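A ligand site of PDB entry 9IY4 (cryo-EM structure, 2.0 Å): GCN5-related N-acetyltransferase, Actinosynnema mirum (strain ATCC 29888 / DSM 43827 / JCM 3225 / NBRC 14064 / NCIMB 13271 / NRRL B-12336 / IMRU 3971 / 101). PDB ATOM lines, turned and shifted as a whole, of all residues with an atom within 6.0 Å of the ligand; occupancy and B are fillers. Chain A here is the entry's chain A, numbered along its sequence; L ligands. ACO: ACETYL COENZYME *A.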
ATOM      1  N   SER A  37     -17.256  20.174  24.753  1.00  0.00           N
ATOM      2  CA  SER A  37     -18.710  20.218  24.910  1.00  0.00           C
ATOM      3  C   SER A  37     -19.419  19.985  23.577  1.00  0.00           C
ATOM      4  O   SER A  37     -20.434  19.274  23.530  1.00  0.00           O
ATOM      5  CB  SER A  37     -19.125  21.561  25.515  1.00  0.00           C
ATOM      6  OG  SER A  37     -18.609  21.697  26.825  1.00  0.00           O
ATOM      7  N   VAL A  38     -18.900  20.564  22.500  1.00  0.00           N
ATOM      8  CA  VAL A  38     -19.494  20.340  21.185  1.00  0.00           C
ATOM      9  C   VAL A  38     -19.285  18.893  20.747  1.00  0.00           C
ATOM     10  O   VAL A  38     -20.164  18.294  20.124  1.00  0.00           O
ATOM     11  CB  VAL A  38     -18.912  21.326  20.164  1.00  0.00           C
ATOM     12  CG1 VAL A  38     -19.395  21.007  18.773  1.00  0.00           C
ATOM     13  CG2 VAL A  38     -19.300  22.729  20.536  1.00  0.00           C
ATOM     14  N   GLY A  41     -21.925  16.964  22.612  1.00  0.00           N
ATOM     15  CA  GLY A  41     -23.266  17.217  22.106  1.00  0.00           C
ATOM     16  C   GLY A  41     -23.510  16.604  20.738  1.00  0.00           C
ATOM     17  O   GLY A  41     -24.542  15.964  20.516  1.00  0.00           O
ATOM     18  N   TYR A  42     -22.568  16.784  19.813  1.00  0.00           N
ATOM     19  CA  TYR A  42     -22.685  16.172  18.493  1.00  0.00           C
ATOM     20  C   TYR A  42     -22.549  14.658  18.567  1.00  0.00           C
ATOM     21  O   TYR A  42     -23.148  13.949  17.758  1.00  0.00           O
ATOM     22  CB  TYR A  42     -21.602  16.718  17.557  1.00  0.00           C
ATOM     23  CG  TYR A  42     -21.931  18.013  16.860  1.00  0.00           C
ATOM     24  CD1 TYR A  42     -23.058  18.744  17.196  1.00  0.00           C
ATOM     25  CD2 TYR A  42     -21.108  18.502  15.869  1.00  0.00           C
ATOM     26  CE1 TYR A  42     -23.346  19.926  16.557  1.00  0.00           C
ATOM     27  CE2 TYR A  42     -21.394  19.689  15.217  1.00  0.00           C
ATOM     28  CZ  TYR A  42     -22.516  20.396  15.575  1.00  0.00           C
ATOM     29  OH  TYR A  42     -22.796  21.578  14.930  1.00  0.00           O
ATOM     30  N   PHE A  99     -30.766  19.474  10.051  1.00  0.00           N
ATOM     31  CA  PHE A  99     -30.276  20.682  10.690  1.00  0.00           C
ATOM     32  C   PHE A  99     -29.319  20.339  11.831  1.00  0.00           C
ATOM     33  O   PHE A  99     -29.599  19.468  12.644  1.00  0.00           O
ATOM     34  CB  PHE A  99     -31.461  21.491  11.214  1.00  0.00           C
ATOM     35  CG  PHE A  99     -31.086  22.609  12.137  1.00  0.00           C
ATOM     36  CD1 PHE A  99     -30.575  23.784  11.632  1.00  0.00           C
ATOM     37  CD2 PHE A  99     -31.259  22.482  13.498  1.00  0.00           C
ATOM     38  CE1 PHE A  99     -30.236  24.815  12.472  1.00  0.00           C
ATOM     39  CE2 PHE A  99     -30.920  23.513  14.338  1.00  0.00           C
ATOM     40  CZ  PHE A  99     -30.405  24.680  13.822  1.00  0.00           C
ATOM     41  N   VAL A 100     -28.179  21.043  11.874  1.00  0.00           N
ATOM     42  CA  VAL A 100     -27.242  20.976  12.991  1.00  0.00           C
ATOM     43  C   VAL A 100     -26.820  22.397  13.368  1.00  0.00           C
ATOM     44  O   VAL A 100     -26.882  23.321  12.548  1.00  0.00           O
ATOM     45  CB  VAL A 100     -26.005  20.116  12.674  1.00  0.00           C
ATOM     46  CG1 VAL A 100     -26.410  18.685  12.398  1.00  0.00           C
ATOM     47  CG2 VAL A 100     -25.243  20.694  11.499  1.00  0.00           C
ATOM     48  N   ILE A 101     -26.375  22.560  14.606  1.00  0.00           N
ATOM     49  CA  ILE A 101     -26.005  23.885  15.118  1.00  0.00           C
ATOM     50  C   ILE A 101     -25.045  23.701  16.290  1.00  0.00           C
ATOM     51  O   ILE A 101     -25.177  22.757  17.074  1.00  0.00           O
ATOM     52  CB  ILE A 101     -27.264  24.692  15.534  1.00  0.00           C
ATOM     53  CG1 ILE A 101     -26.881  26.041  16.130  1.00  0.00           C
ATOM     54  CG2 ILE A 101     -28.095  23.908  16.512  1.00  0.00           C
ATOM     55  CD1 ILE A 101     -28.039  26.985  16.295  1.00  0.00           C
ATOM     56  N   GLN A 102     -24.067  24.604  16.399  1.00  0.00           N
ATOM     57  CA  GLN A 102     -23.255  24.717  17.596  1.00  0.00           C
ATOM     58  C   GLN A 102     -22.805  26.161  17.768  1.00  0.00           C
ATOM     59  O   GLN A 102     -22.572  26.872  16.791  1.00  0.00           O
ATOM     60  CB  GLN A 102     -22.030  23.797  17.547  1.00  0.00           C
ATOM     61  CG  GLN A 102     -21.090  24.016  16.381  1.00  0.00           C
ATOM     62  CD  GLN A 102     -20.047  25.069  16.661  1.00  0.00           C
ATOM     63  OE1 GLN A 102     -19.626  25.240  17.804  1.00  0.00           O
ATOM     64  NE2 GLN A 102     -19.612  25.771  15.630  1.00  0.00           N
ATOM     65  N   LEU A 103     -22.689  26.580  19.028  1.00  0.00           N
ATOM     66  CA  LEU A 103     -22.168  27.898  19.377  1.00  0.00           C
ATOM     67  C   LEU A 103     -20.848  27.767  20.120  1.00  0.00           C
ATOM     68  O   LEU A 103     -20.493  26.699  20.625  1.00  0.00           O
ATOM     69  CB  LEU A 103     -23.159  28.701  20.222  1.00  0.00           C
ATOM     70  CG  LEU A 103     -24.555  28.949  19.696  1.00  0.00           C
ATOM     71  CD1 LEU A 103     -25.366  29.701  20.731  1.00  0.00           C
ATOM     72  CD2 LEU A 103     -24.478  29.749  18.417  1.00  0.00           C
ATOM     73  N   GLY A 104     -20.124  28.881  20.197  1.00  0.00           N
ATOM     74  CA  GLY A 104     -18.911  28.933  20.978  1.00  0.00           C
ATOM     75  C   GLY A 104     -19.178  28.846  22.464  1.00  0.00           C
ATOM     76  O   GLY A 104     -20.306  28.980  22.938  1.00  0.00           O
ATOM     77  N   HIS A 107     -20.946  31.840  24.463  1.00  0.00           N
ATOM     78  CA  HIS A 107     -22.142  32.448  23.872  1.00  0.00           C
ATOM     79  C   HIS A 107     -23.408  31.646  24.162  1.00  0.00           C
ATOM     80  O   HIS A 107     -24.482  32.015  23.661  1.00  0.00           O
ATOM     81  CB  HIS A 107     -21.949  32.598  22.361  1.00  0.00           C
ATOM     82  CG  HIS A 107     -20.691  33.310  21.976  1.00  0.00           C
ATOM     83  ND1 HIS A 107     -20.479  34.641  22.259  1.00  0.00           N
ATOM     84  CD2 HIS A 107     -19.589  32.886  21.324  1.00  0.00           C
ATOM     85  CE1 HIS A 107     -19.294  35.001  21.809  1.00  0.00           C
ATOM     86  NE2 HIS A 107     -18.733  33.959  21.228  1.00  0.00           N
ATOM     87  N   ARG A 108     -23.323  30.598  24.955  1.00  0.00           N
ATOM     88  CA  ARG A 108     -24.462  29.731  25.239  1.00  0.00           C
ATOM     89  C   ARG A 108     -25.229  30.222  26.458  1.00  0.00           C
ATOM     90  O   ARG A 108     -24.662  30.805  27.378  1.00  0.00           O
ATOM     91  CB  ARG A 108     -24.007  28.300  25.462  1.00  0.00           C
ATOM     92  CG  ARG A 108     -23.267  27.716  24.285  1.00  0.00           C
ATOM     93  CD  ARG A 108     -22.458  26.503  24.690  1.00  0.00           C
ATOM     94  NE  ARG A 108     -21.506  26.140  23.647  1.00  0.00           N
ATOM     95  CZ  ARG A 108     -20.437  25.385  23.846  1.00  0.00           C
ATOM     96  NH1 ARG A 108     -20.153  24.891  25.034  1.00  0.00           N
ATOM     97  NH2 ARG A 108     -19.634  25.128  22.814  1.00  0.00           N
ATOM     98  N   GLY A 109     -26.526  29.963  26.455  1.00  0.00           N
ATOM     99  CA  GLY A 109     -27.409  30.413  27.510  1.00  0.00           C
ATOM    100  C   GLY A 109     -27.902  31.828  27.367  1.00  0.00           C
ATOM    101  O   GLY A 109     -28.709  32.270  28.197  1.00  0.00           O
ATOM    102  N   ARG A 110     -27.459  32.557  26.350  1.00  0.00           N
ATOM    103  CA  ARG A 110     -27.893  33.922  26.102  1.00  0.00           C
ATOM    104  C   ARG A 110     -29.010  34.012  25.064  1.00  0.00           C
ATOM    105  O   ARG A 110     -29.431  35.116  24.720  1.00  0.00           O
ATOM    106  CB  ARG A 110     -26.711  34.794  25.663  1.00  0.00           C
ATOM    107  CG  ARG A 110     -25.717  35.091  26.762  1.00  0.00           C
ATOM    108  CD  ARG A 110     -24.369  35.435  26.161  1.00  0.00           C
ATOM    109  NE  ARG A 110     -24.464  36.553  25.233  1.00  0.00           N
ATOM    110  CZ  ARG A 110     -23.519  36.889  24.368  1.00  0.00           C
ATOM    111  NH1 ARG A 110     -22.395  36.204  24.271  1.00  0.00           N
ATOM    112  NH2 ARG A 110     -23.700  37.942  23.584  1.00  0.00           N
ATOM    113  N   GLY A 111     -29.486  32.873  24.559  1.00  0.00           N
ATOM    114  CA  GLY A 111     -30.585  32.854  23.633  1.00  0.00           C
ATOM    115  C   GLY A 111     -30.210  32.825  22.163  1.00  0.00           C
ATOM    116  O   GLY A 111     -31.090  32.586  21.337  1.00  0.00           O
ATOM    117  N   LEU A 112     -28.932  33.030  21.818  1.00  0.00           N
ATOM    118  CA  LEU A 112     -28.555  33.157  20.409  1.00  0.00           C
ATOM    119  C   LEU A 112     -28.883  31.908  19.600  1.00  0.00           C
ATOM    120  O   LEU A 112     -29.167  32.007  18.404  1.00  0.00           O
ATOM    121  CB  LEU A 112     -27.066  33.463  20.302  1.00  0.00           C
ATOM    122  CG  LEU A 112     -26.624  34.806  20.890  1.00  0.00           C
ATOM    123  CD1 LEU A 112     -25.114  34.886  20.938  1.00  0.00           C
ATOM    124  CD2 LEU A 112     -27.205  35.959  20.093  1.00  0.00           C
ATOM    125  N   GLY A 113     -28.846  30.737  20.229  1.00  0.00           N
ATOM    126  CA  GLY A 113     -29.152  29.514  19.515  1.00  0.00           C
ATOM    127  C   GLY A 113     -30.594  29.448  19.039  1.00  0.00           C
ATOM    128  O   GLY A 113     -30.882  28.960  17.945  1.00  0.00           O
ATOM    129  N   THR A 114     -31.528  29.952  19.857  1.00  0.00           N
ATOM    130  CA  THR A 114     -32.938  29.920  19.504  1.00  0.00           C
ATOM    131  C   THR A 114     -33.226  30.752  18.251  1.00  0.00           C
ATOM    132  O   THR A 114     -33.827  30.258  17.294  1.00  0.00           O
ATOM    133  CB  THR A 114     -33.784  30.417  20.672  1.00  0.00           C
ATOM    134  OG1 THR A 114     -33.562  29.583  21.809  1.00  0.00           O
ATOM    135  CG2 THR A 114     -35.256  30.359  20.319  1.00  0.00           C
ATOM    136  N   GLU A 115     -32.789  32.024  18.237  1.00  0.00           N
ATOM    137  CA  GLU A 115     -33.019  32.836  17.056  1.00  0.00           C
ATOM    138  C   GLU A 115     -32.161  32.411  15.875  1.00  0.00           C
ATOM    139  O   GLU A 115     -32.570  32.585  14.736  1.00  0.00           O
ATOM    140  CB  GLU A 115     -32.831  34.329  17.336  1.00  0.00           C
ATOM    141  CG  GLU A 115     -33.871  34.941  18.269  1.00  0.00           C
ATOM    142  CD  GLU A 115     -33.588  34.733  19.730  1.00  0.00           C
ATOM    143  OE1 GLU A 115     -32.541  34.152  20.040  1.00  0.00           O
ATOM    144  OE2 GLU A 115     -34.419  35.128  20.575  1.00  0.00           O
ATOM    145  N   LEU A 135     -34.011  17.042  12.667  1.00  0.00           N
ATOM    146  CA  LEU A 135     -32.747  16.963  13.392  1.00  0.00           C
ATOM    147  C   LEU A 135     -32.739  15.726  14.268  1.00  0.00           C
ATOM    148  O   LEU A 135     -33.796  15.171  14.594  1.00  0.00           O
ATOM    149  CB  LEU A 135     -32.497  18.225  14.231  1.00  0.00           C
ATOM    150  CG  LEU A 135     -33.481  18.629  15.332  1.00  0.00           C
ATOM    151  CD1 LEU A 135     -33.278  17.875  16.627  1.00  0.00           C
ATOM    152  CD2 LEU A 135     -33.408  20.115  15.565  1.00  0.00           C
ATOM    153  N   ALA A 136     -31.540  15.302  14.650  1.00  0.00           N
ATOM    154  CA  ALA A 136     -31.340  14.248  15.634  1.00  0.00           C
ATOM    155  C   ALA A 136     -30.455  14.790  16.741  1.00  0.00           C
ATOM    156  O   ALA A 136     -29.369  15.324  16.482  1.00  0.00           O
ATOM    157  CB  ALA A 136     -30.702  13.021  14.993  1.00  0.00           C
ATOM    158  N   VAL A 137     -30.922  14.654  17.974  1.00  0.00           N
ATOM    159  CA  VAL A 137     -30.258  15.231  19.144  1.00  0.00           C
ATOM    160  C   VAL A 137     -30.261  14.209  20.276  1.00  0.00           C
ATOM    161  O   VAL A 137     -31.276  13.540  20.521  1.00  0.00           O
ATOM    162  CB  VAL A 137     -30.930  16.560  19.557  1.00  0.00           C
ATOM    163  CG1 VAL A 137     -32.336  16.318  19.995  1.00  0.00           C
ATOM    164  CG2 VAL A 137     -30.180  17.206  20.693  1.00  0.00           C
ATOM    165  N   LEU A 138     -29.126  14.084  20.950  1.00  0.00           N
ATOM    166  CA  LEU A 138     -29.031  13.167  22.084  1.00  0.00           C
ATOM    167  C   LEU A 138     -29.982  13.600  23.196  1.00  0.00           C
ATOM    168  O   LEU A 138     -30.087  14.785  23.524  1.00  0.00           O
ATOM    169  CB  LEU A 138     -27.594  13.116  22.609  1.00  0.00           C
ATOM    170  CG  LEU A 138     -26.544  12.532  21.659  1.00  0.00           C
ATOM    171  CD1 LEU A 138     -25.160  12.711  22.229  1.00  0.00           C
ATOM    172  CD2 LEU A 138     -26.818  11.070  21.401  1.00  0.00           C
ATOM    173  N   ASN A 141     -29.191  16.012  26.160  1.00  0.00           N
ATOM    174  CA  ASN A 141     -28.889  17.384  25.758  1.00  0.00           C
ATOM    175  C   ASN A 141     -30.178  18.212  25.802  1.00  0.00           C
ATOM    176  O   ASN A 141     -30.738  18.617  24.776  1.00  0.00           O
ATOM    177  CB  ASN A 141     -28.247  17.390  24.383  1.00  0.00           C
ATOM    178  CG  ASN A 141     -27.632  18.717  24.017  1.00  0.00           C
ATOM    179  OD1 ASN A 141     -27.953  19.739  24.610  1.00  0.00           O
ATOM    180  ND2 ASN A 141     -26.757  18.706  23.028  1.00  0.00           N
ATOM    181  N   THR A 142     -30.649  18.459  27.022  1.00  0.00           N
ATOM    182  CA  THR A 142     -31.971  19.058  27.218  1.00  0.00           C
ATOM    183  C   THR A 142     -32.019  20.524  26.802  1.00  0.00           C
ATOM    184  O   THR A 142     -33.070  21.001  26.352  1.00  0.00           O
ATOM    185  CB  THR A 142     -32.410  18.911  28.662  1.00  0.00           C
ATOM    186  OG1 THR A 142     -31.402  19.463  29.523  1.00  0.00           O
ATOM    187  CG2 THR A 142     -32.605  17.455  29.016  1.00  0.00           C
ATOM    188  N   GLY A 143     -30.924  21.254  26.966  1.00  0.00           N
ATOM    189  CA  GLY A 143     -30.906  22.652  26.548  1.00  0.00           C
ATOM    190  C   GLY A 143     -31.175  22.795  25.068  1.00  0.00           C
ATOM    191  O   GLY A 143     -31.943  23.662  24.644  1.00  0.00           O
ATOM    192  N   ALA A 144     -30.528  21.956  24.254  1.00  0.00           N
ATOM    193  CA  ALA A 144     -30.806  21.954  22.835  1.00  0.00           C
ATOM    194  C   ALA A 144     -32.259  21.598  22.551  1.00  0.00           C
ATOM    195  O   ALA A 144     -32.866  22.151  21.635  1.00  0.00           O
ATOM    196  CB  ALA A 144     -29.866  20.993  22.107  1.00  0.00           C
ATOM    197  N   ALA A 146     -34.932  22.264  24.426  1.00  0.00           N
ATOM    198  CA  ALA A 146     -35.752  23.445  24.677  1.00  0.00           C
ATOM    199  C   ALA A 146     -35.548  24.507  23.606  1.00  0.00           C
ATOM    200  O   ALA A 146     -36.506  25.135  23.137  1.00  0.00           O
ATOM    201  CB  ALA A 146     -35.444  24.006  26.057  1.00  0.00           C
ATOM    202  N   ALA A 147     -34.289  24.719  23.190  1.00  0.00           N
ATOM    203  CA  ALA A 147     -34.016  25.704  22.152  1.00  0.00           C
ATOM    204  C   ALA A 147     -34.713  25.338  20.842  1.00  0.00           C
ATOM    205  O   ALA A 147     -35.318  26.205  20.189  1.00  0.00           O
ATOM    206  CB  ALA A 147     -32.508  25.826  21.930  1.00  0.00           C
ATOM    207  N   TYR A 148     -34.659  24.069  20.462  1.00  0.00           N
ATOM    208  CA  TYR A 148     -35.307  23.637  19.226  1.00  0.00           C
ATOM    209  C   TYR A 148     -36.821  23.741  19.327  1.00  0.00           C
ATOM    210  O   TYR A 148     -37.479  24.107  18.352  1.00  0.00           O
ATOM    211  CB  TYR A 148     -34.886  22.202  18.894  1.00  0.00           C
ATOM    212  CG  TYR A 148     -33.409  22.012  18.708  1.00  0.00           C
ATOM    213  CD1 TYR A 148     -32.594  23.055  18.302  1.00  0.00           C
ATOM    214  CD2 TYR A 148     -32.820  20.783  18.950  1.00  0.00           C
ATOM    215  CE1 TYR A 148     -31.234  22.874  18.131  1.00  0.00           C
ATOM    216  CE2 TYR A 148     -31.463  20.597  18.792  1.00  0.00           C
ATOM    217  CZ  TYR A 148     -30.678  21.641  18.381  1.00  0.00           C
ATOM    218  OH  TYR A 148     -29.336  21.432  18.234  1.00  0.00           O
ATOM    219  N   ARG A 150     -38.614  25.882  21.129  1.00  0.00           N
ATOM    220  CA  ARG A 150     -39.033  27.274  20.981  1.00  0.00           C
ATOM    221  C   ARG A 150     -38.726  27.830  19.606  1.00  0.00           C
ATOM    222  O   ARG A 150     -39.413  28.752  19.158  1.00  0.00           O
ATOM    223  CB  ARG A 150     -38.406  28.137  22.074  1.00  0.00           C
ATOM    224  CG  ARG A 150     -39.362  28.373  23.232  1.00  0.00           C
ATOM    225  CD  ARG A 150     -38.821  29.331  24.288  1.00  0.00           C
ATOM    226  NE  ARG A 150     -38.044  28.652  25.312  1.00  0.00           N
ATOM    227  CZ  ARG A 150     -36.716  28.605  25.366  1.00  0.00           C
ATOM    228  NH1 ARG A 150     -35.978  29.175  24.435  1.00  0.00           N
ATOM    229  NH2 ARG A 150     -36.138  27.976  26.384  1.00  0.00           N
HETATM  230  N1A ACO L   1     -31.396  22.057  31.197  1.00  0.00           N
HETATM  231  C2A ACO L   1     -32.618  22.403  30.847  1.00  0.00           C
HETATM  232  N3A ACO L   1     -32.870  23.494  30.152  1.00  0.00           N
HETATM  233  C4A ACO L   1     -31.888  24.294  29.763  1.00  0.00           C
HETATM  234  C5A ACO L   1     -30.567  23.974  30.111  1.00  0.00           C
HETATM  235  C6A ACO L   1     -30.347  22.797  30.857  1.00  0.00           C
HETATM  236  N6A ACO L   1     -29.064  22.417  31.234  1.00  0.00           N
HETATM  237  N7A ACO L   1     -29.769  24.945  29.600  1.00  0.00           N
HETATM  238  C8A ACO L   1     -30.501  25.816  28.981  1.00  0.00           C
HETATM  239  N9A ACO L   1     -31.818  25.465  29.059  1.00  0.00           N
HETATM  240  C1B ACO L   1     -32.947  26.197  28.480  1.00  0.00           C
HETATM  241  C2B ACO L   1     -32.945  27.667  28.959  1.00  0.00           C
HETATM  242  O2B ACO L   1     -34.235  28.021  29.483  1.00  0.00           O
HETATM  243  C3B ACO L   1     -32.627  28.492  27.695  1.00  0.00           C
HETATM  244  O3B ACO L   1     -33.449  29.668  27.654  1.00  0.00           O
HETATM  245  P3B ACO L   1     -32.466  30.941  27.793  1.00  0.00           P
HETATM  246  O7A ACO L   1     -32.786  31.672  29.040  1.00  0.00           O
HETATM  247  O8A ACO L   1     -30.932  30.464  27.837  1.00  0.00           O
HETATM  248  O9A ACO L   1     -32.677  31.925  26.535  1.00  0.00           O
HETATM  249  C4B ACO L   1     -33.016  27.534  26.557  1.00  0.00           C
HETATM  250  O4B ACO L   1     -32.805  26.210  27.041  1.00  0.00           O
HETATM  251  C5B ACO L   1     -32.140  27.760  25.327  1.00  0.00           C
HETATM  252  O5B ACO L   1     -31.621  29.092  25.322  1.00  0.00           O
HETATM  253  P1A ACO L   1     -30.530  29.125  24.141  1.00  0.00           P
HETATM  254  O1A ACO L   1     -29.347  29.886  24.577  1.00  0.00           O
HETATM  255  O2A ACO L   1     -31.165  29.829  22.849  1.00  0.00           O
HETATM  256  O3A ACO L   1     -30.151  27.613  23.783  1.00  0.00           O
HETATM  257  P2A ACO L   1     -28.561  27.487  23.600  1.00  0.00           P
HETATM  258  O4A ACO L   1     -27.883  27.693  24.891  1.00  0.00           O
HETATM  259  O5A ACO L   1     -28.062  28.573  22.530  1.00  0.00           O
HETATM  260  O6A ACO L   1     -28.216  25.997  23.105  1.00  0.00           O
HETATM  261  CBP ACO L   1     -26.981  25.097  21.275  1.00  0.00           C
HETATM  262  CCP ACO L   1     -28.162  25.975  21.681  1.00  0.00           C
HETATM  263  CDP ACO L   1     -26.646  25.374  19.807  1.00  0.00           C
HETATM  264  CEP ACO L   1     -27.379  23.634  21.456  1.00  0.00           C
HETATM  265  CAP ACO L   1     -25.794  25.443  22.188  1.00  0.00           C
HETATM  266  OAP ACO L   1     -26.162  25.213  23.538  1.00  0.00           O
HETATM  267  C9P ACO L   1     -24.537  24.656  21.898  1.00  0.00           C
HETATM  268  O9P ACO L   1     -23.768  25.026  21.040  1.00  0.00           O
HETATM  269  N8P ACO L   1     -24.241  23.564  22.632  1.00  0.00           N
HETATM  270  C7P ACO L   1     -23.019  22.773  22.443  1.00  0.00           C
HETATM  271  C6P ACO L   1     -23.010  21.969  21.139  1.00  0.00           C
HETATM  272  C5P ACO L   1     -24.360  21.364  20.953  1.00  0.00           C
HETATM  273  O5P ACO L   1     -24.971  20.937  21.907  1.00  0.00           O
HETATM  274  N4P ACO L   1     -24.899  21.296  19.731  1.00  0.00           N
HETATM  275  C3P ACO L   1     -26.226  20.695  19.590  1.00  0.00           C
HETATM  276  C2P ACO L   1     -26.114  19.376  18.846  1.00  0.00           C
HETATM  277  S1P ACO L   1     -27.788  18.715  18.764  1.00  0.00           S
HETATM  278  C   ACO L   1     -27.791  18.213  17.144  1.00  0.00           C
HETATM  279  O   ACO L   1     -27.198  17.191  16.828  1.00  0.00           O
HETATM  280  CH3 ACO L   1     -28.525  19.031  16.118  1.00  0.00           C
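The backbone NH (N) of Gly 113 lies within hydrogen-bond range of an oxygen (O5A) of the ligand, 3.3 Å away.
The backbone NH of Leu 103 sits at hydrogen-bond distance from an oxygen (O9P) of the ligand (2.8 Å).
The backbone NH (N) of Thr 114 is in hydrogen-bond range of an oxygen (O2A) of the ligand (3.0 Å).
S1P of the ligand lies close to OH of Tyr 148, at 3.2 Å.
The side-chain hydroxyl (OG1) of Thr 142 sits at hydrogen-bond distance from a nitrogen (N1A) of the ligand (3.1 Å).
An oxygen (O4A) of the ligand is in hydrogen-bond range of the backbone NH (N) of Gly 109, at 3.1 Å.
The backbone NH (N) of Gly 111 is in hydrogen-bond range of an oxygen (O1A) of the ligand (3.0 Å).
The guanidinium group of Arg 150 lies close to an oxygen (O3B) of the ligand (3.4 Å).
OG1 of Thr 114 is in hydrogen-bond range of O2A of the ligand (2.6 Å).
The backbone carbonyl oxygen of Gly 109 sits close to an oxygen (O8A) of the ligand (2.9 Å).
A nitrogen (N4P) of the ligand sits at hydrogen-bond distance from the backbone carbonyl oxygen (O) of Ile 101, at 3.0 Å.
O5P of the ligand sits at hydrogen-bond distance from ND2 of Asn 141 (3.1 Å).
The guanidinium group (NE) of Arg 108 is in hydrogen-bond range of the backbone carbonyl oxygen (O) of Gly 104, 3.2 Å away.
A ring nitrogen (ND1) of His 107 sits at hydrogen-bond distance from the guanidinium group (NH1) of Arg 110, 3.2 Å away.
O of Leu 103 is in hydrogen-bond range of NH2 of Arg 108 (2.8 Å).
The side-chain carboxylate of Glu 115 sits close to the backbone carbonyl oxygen of Gly 111, at 2.5 Å.
The side-chain amide oxygen of Asn 141 sits close to the backbone NH of Ala 144, at 3.4 Å.
The side-chain hydroxyl (OH) of Tyr 42 lies close to the backbone carbonyl oxygen (O) of Ile 101, 3.4 Å away.
O of Ala 136 lies close to O of the ligand (2.9 Å).
Val 38 touches the ligand (CG2 to C6P, 3.8 Å).
Tyr 42 touches the ligand (CD1 to C2P, 3.5 Å).
Phe 99 touches the ligand.
Val 100 touches the ligand.
CA of Gln 102 touches O9P of the ligand, at 3.5 Å.
Arg 108 touches the ligand.
N of Arg 110 touches O1A of the ligand, 3.7 Å away.
CG2 of Val 137 touches S1P of the ligand, 3.4 Å away.
O of Gly 143 touches O4B of the ligand (3.6 Å).
Ala 144 touches the ligand.
CB of Ala 146 touches O4B of the ligand, 3.6 Å away.
Ala 147 touches the ligand (CB to O3A, 3.5 Å).
Hydrophobic or aromatic side chains that line the ligand: Val 38, Tyr 42, Ile 101, Leu 103, Val 137, Ala 144, Ala 146 and Ala 147.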
